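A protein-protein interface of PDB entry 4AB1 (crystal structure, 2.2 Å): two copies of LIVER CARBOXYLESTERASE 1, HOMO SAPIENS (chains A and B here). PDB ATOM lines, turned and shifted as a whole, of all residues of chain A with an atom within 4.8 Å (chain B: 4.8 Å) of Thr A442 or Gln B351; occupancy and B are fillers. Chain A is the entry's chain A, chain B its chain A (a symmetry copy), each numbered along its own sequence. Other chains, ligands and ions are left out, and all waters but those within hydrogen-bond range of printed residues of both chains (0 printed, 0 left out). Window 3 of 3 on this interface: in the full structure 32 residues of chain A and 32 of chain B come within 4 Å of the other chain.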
ATOM      1  N   GLN A 333      -3.211 -30.475  -6.790  1.00  0.00           N
ATOM      2  CA  GLN A 333      -3.692 -29.395  -5.947  1.00  0.00           C
ATOM      3  C   GLN A 333      -4.974 -28.762  -6.541  1.00  0.00           C
ATOM      4  O   GLN A 333      -4.981 -27.604  -7.003  1.00  0.00           O
ATOM      5  CB  GLN A 333      -2.600 -28.336  -5.665  1.00  0.00           C
ATOM      6  CG  GLN A 333      -1.351 -28.807  -4.875  1.00  0.00           C
ATOM      7  CD  GLN A 333      -0.358 -27.632  -4.686  1.00  0.00           C
ATOM      8  OE1 GLN A 333      -0.762 -26.489  -4.619  1.00  0.00           O
ATOM      9  NE2 GLN A 333       0.903 -27.908  -4.682  1.00  0.00           N
ATOM     10  N   ASP A 394      -2.282 -25.050   3.757  1.00  0.00           N
ATOM     11  CA  ASP A 394      -2.129 -25.946   2.601  1.00  0.00           C
ATOM     12  C   ASP A 394      -3.081 -27.125   2.831  1.00  0.00           C
ATOM     13  O   ASP A 394      -3.850 -27.495   1.927  1.00  0.00           O
ATOM     14  CB  ASP A 394      -0.692 -26.472   2.492  1.00  0.00           C
ATOM     15  CG  ASP A 394       0.250 -25.457   1.920  1.00  0.00           C
ATOM     16  OD1 ASP A 394      -0.244 -24.543   1.241  1.00  0.00           O
ATOM     17  OD2 ASP A 394       1.488 -25.580   2.148  1.00  0.00           O
ATOM     18  N   PRO A 440       1.282 -18.264  -7.651  1.00  0.00           N
ATOM     19  CA  PRO A 440       2.533 -18.389  -6.914  1.00  0.00           C
ATOM     20  C   PRO A 440       3.205 -19.684  -7.358  1.00  0.00           C
ATOM     21  O   PRO A 440       2.504 -20.640  -7.738  1.00  0.00           O
ATOM     22  CB  PRO A 440       2.077 -18.439  -5.423  1.00  0.00           C
ATOM     23  CG  PRO A 440       0.596 -18.078  -5.417  1.00  0.00           C
ATOM     24  CD  PRO A 440       0.083 -18.406  -6.795  1.00  0.00           C
ATOM     25  N   LYS A 441       4.539 -19.664  -7.375  1.00  0.00           N
ATOM     26  CA  LYS A 441       5.438 -20.794  -7.711  1.00  0.00           C
ATOM     27  C   LYS A 441       5.123 -22.129  -7.032  1.00  0.00           C
ATOM     28  O   LYS A 441       5.234 -23.173  -7.650  1.00  0.00           O
ATOM     29  CB  LYS A 441       6.899 -20.412  -7.324  1.00  0.00           C
ATOM     30  CG  LYS A 441       7.886 -20.233  -8.464  1.00  0.00           C
ATOM     31  N   THR A 442       4.809 -22.114  -5.742  1.00  0.00           N
ATOM     32  CA  THR A 442       4.598 -23.369  -5.019  1.00  0.00           C
ATOM     33  C   THR A 442       3.332 -24.180  -5.459  1.00  0.00           C
ATOM     34  O   THR A 442       3.162 -25.348  -5.090  1.00  0.00           O
ATOM     35  CB  THR A 442       4.588 -23.139  -3.491  1.00  0.00           C
ATOM     36  OG1 THR A 442       3.494 -22.293  -3.127  1.00  0.00           O
ATOM     37  CG2 THR A 442       5.918 -22.474  -3.069  1.00  0.00           C
ATOM     38  N   VAL A 443       2.436 -23.582  -6.236  1.00  0.00           N
ATOM     39  CA  VAL A 443       1.245 -24.359  -6.657  1.00  0.00           C
ATOM     40  C   VAL A 443       1.621 -25.292  -7.783  1.00  0.00           C
ATOM     41  O   VAL A 443       2.201 -24.878  -8.810  1.00  0.00           O
ATOM     42  CB  VAL A 443       0.048 -23.444  -7.006  1.00  0.00           C
ATOM     43  CG1 VAL A 443      -1.172 -24.279  -7.435  1.00  0.00           C
ATOM     44  CG2 VAL A 443      -0.263 -22.620  -5.765  1.00  0.00           C
ATOM     45  N   ILE A 444       1.351 -26.573  -7.577  1.00  0.00           N
ATOM     46  CA  ILE A 444       1.729 -27.558  -8.593  1.00  0.00           C
ATOM     47  C   ILE A 444       0.483 -28.461  -8.921  1.00  0.00           C
ATOM     48  O   ILE A 444      -0.193 -28.924  -8.014  1.00  0.00           O
ATOM     49  CB  ILE A 444       3.072 -28.308  -8.186  1.00  0.00           C
ATOM     50  CG1 ILE A 444       4.262 -27.283  -8.146  1.00  0.00           C
ATOM     51  CG2 ILE A 444       3.356 -29.460  -9.133  1.00  0.00           C
ATOM     52  CD1 ILE A 444       5.507 -27.571  -7.279  1.00  0.00           C
ATOM     53  N   GLU B 349      -3.073 -18.255  -1.532  1.00  0.00           N
ATOM     54  CA  GLU B 349      -1.966 -19.133  -1.157  1.00  0.00           C
ATOM     55  C   GLU B 349      -1.244 -18.659   0.069  1.00  0.00           C
ATOM     56  O   GLU B 349      -0.638 -19.453   0.834  1.00  0.00           O
ATOM     57  CB  GLU B 349      -0.949 -19.233  -2.297  1.00  0.00           C
ATOM     58  CG  GLU B 349      -1.145 -20.492  -3.124  1.00  0.00           C
ATOM     59  CD  GLU B 349      -0.659 -21.764  -2.422  1.00  0.00           C
ATOM     60  OE1 GLU B 349       0.574 -21.849  -2.110  1.00  0.00           O
ATOM     61  OE2 GLU B 349      -1.515 -22.678  -2.237  1.00  0.00           O
ATOM     62  N   GLY B 350      -1.265 -17.346   0.215  1.00  0.00           N
ATOM     63  CA  GLY B 350      -0.612 -16.698   1.327  1.00  0.00           C
ATOM     64  C   GLY B 350       0.884 -16.810   1.320  1.00  0.00           C
ATOM     65  O   GLY B 350       1.523 -16.735   2.359  1.00  0.00           O
ATOM     66  N   GLN B 351       1.442 -17.005   0.143  1.00  0.00           N
ATOM     67  CA  GLN B 351       2.887 -16.849  -0.022  1.00  0.00           C
ATOM     68  C   GLN B 351       3.219 -16.268  -1.390  1.00  0.00           C
ATOM     69  O   GLN B 351       2.358 -16.283  -2.298  1.00  0.00           O
ATOM     70  CB  GLN B 351       3.678 -18.121   0.303  1.00  0.00           C
ATOM     71  CG  GLN B 351       2.888 -19.410   0.227  1.00  0.00           C
ATOM     72  CD  GLN B 351       3.723 -20.651   0.510  1.00  0.00           C
ATOM     73  OE1 GLN B 351       4.911 -20.751   0.157  1.00  0.00           O
ATOM     74  NE2 GLN B 351       3.105 -21.598   1.140  1.00  0.00           N
ATOM     75  N   LEU B 352       4.439 -15.731  -1.507  1.00  0.00           N
ATOM     76  CA  LEU B 352       4.805 -14.900  -2.659  1.00  0.00           C
ATOM     77  C   LEU B 352       6.266 -14.973  -2.904  1.00  0.00           C
ATOM     78  O   LEU B 352       7.055 -14.699  -2.015  1.00  0.00           O
ATOM     79  CB  LEU B 352       4.440 -13.446  -2.434  1.00  0.00           C
ATOM     80  CG  LEU B 352       3.626 -12.707  -3.503  1.00  0.00           C
ATOM     81  CD1 LEU B 352       2.247 -13.303  -3.818  1.00  0.00           C
ATOM     82  CD2 LEU B 352       3.429 -11.293  -2.979  1.00  0.00           C
ATOM     83  N   ASP B 353       6.604 -15.395  -4.119  1.00  0.00           N
ATOM     84  CA  ASP B 353       7.942 -15.278  -4.694  1.00  0.00           C
ATOM     85  C   ASP B 353       7.981 -13.927  -5.340  1.00  0.00           C
ATOM     86  O   ASP B 353       6.921 -13.346  -5.638  1.00  0.00           O
ATOM     87  CB  ASP B 353       8.150 -16.363  -5.763  1.00  0.00           C
ATOM     88  CG  ASP B 353       6.999 -16.415  -6.785  1.00  0.00           C
ATOM     89  OD1 ASP B 353       5.855 -16.900  -6.496  1.00  0.00           O
ATOM     90  OD2 ASP B 353       7.261 -15.963  -7.886  1.00  0.00           O
ATOM     91  N   THR B 389       8.952 -16.829   1.667  1.00  0.00           N
ATOM     92  CA  THR B 389       7.807 -16.340   0.834  1.00  0.00           C
ATOM     93  C   THR B 389       6.502 -15.987   1.603  1.00  0.00           C
ATOM     94  O   THR B 389       5.596 -15.369   1.016  1.00  0.00           O
ATOM     95  CB  THR B 389       7.398 -17.285  -0.376  1.00  0.00           C
ATOM     96  OG1 THR B 389       6.863 -18.543   0.097  1.00  0.00           O
ATOM     97  CG2 THR B 389       8.546 -17.476  -1.383  1.00  0.00           C
ATOM     98  N   VAL B 390       6.391 -16.444   2.857  1.00  0.00           N
ATOM     99  CA  VAL B 390       5.284 -16.092   3.770  1.00  0.00           C
ATOM    100  C   VAL B 390       5.467 -14.637   4.275  1.00  0.00           C
ATOM    101  O   VAL B 390       4.540 -13.810   4.155  1.00  0.00           O
ATOM    102  CB  VAL B 390       5.144 -17.065   4.978  1.00  0.00           C
ATOM    103  N   LYS B 393       5.174 -12.175   1.650  1.00  0.00           N
ATOM    104  CA  LYS B 393       3.778 -11.890   1.439  1.00  0.00           C
ATOM    105  C   LYS B 393       3.356 -10.797   2.407  1.00  0.00           C
ATOM    106  O   LYS B 393       2.527  -9.974   2.041  1.00  0.00           O
ATOM    107  CB  LYS B 393       2.856 -13.119   1.574  1.00  0.00           C
ATOM    108  CG  LYS B 393       1.392 -12.846   1.207  1.00  0.00           C
ATOM    109  CD  LYS B 393       0.433 -12.749   2.429  1.00  0.00           C
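OG1 of Thr A442 sits at hydrogen-bond distance from OE1 of Glu B349. N of Lys A441 lies within hydrogen-bond range of OD1 of Asp B353 (3.2 Å).
The side-chain amide nitrogen (NE2) of Gln A333 is in hydrogen-bond range of the backbone carbonyl oxygen (O) of Thr A442 (3.4 Å). The side-chain amide oxygen (OE1) of Gln B351 lies within hydrogen-bond range of the side-chain hydroxyl (OG1) of Thr B389 (2.9 Å).
CB of Glu B349 touches CG of Pro A440 (3.7 Å). Pro A440 touches Gln B351. Asp B353 touches Pro A440. OE1 of Gln B351 touches CG2 of Thr A442 (3.8 Å). CD of Glu B349 touches CG2 of Val A443 (3.5 Å).
Of chain B, only Glu B349 (3.1 Å) and Gln B351 (3.8 Å) come within 4 Å of Thr A442. Of chain A, only Pro A440 and Thr A442 come within 4 Å of Gln B351. Of the printed residues of chain B, Lys A441 touches Asp B353. Printed residues of chain A within 4 Å of Asp B353: Pro A440 (3.7 Å) and Lys A441 (3.2 Å). Of the printed residues of chain B, Val A443 touches Glu B349 (3.5 Å). Printed residues of chain B within 4 Å of Pro A440: Glu B349, Gln B351 and Asp B353. Of the printed residues of chain A, Glu B349 touches Pro A440, Thr A442 and Val A443. The nearest printed residue of chain B that does not touch Thr A442 is Thr B389 (5.1 Å). The nearest residue of chain A that does not touch Gln B351 is Asp A394 (4.4 Å). The nearest printed residue of chain A that does not touch Asp B353 is Thr A442 (5.4 Å).
Of the 7 printed residues of chain A, 4 touch a printed residue of chain B. Hydrophobic or aromatic side chains of chain A that line the printed part of chain B: Pro A440 and Val A443. Of the 8 printed residues of chain B, 3 touch a printed residue of chain A. Among the printed residues, no Asp or Glu carboxylate lies within 4 Å of a Lys or Arg side-chain nitrogen of the other chain.
No position is printed for both chains.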
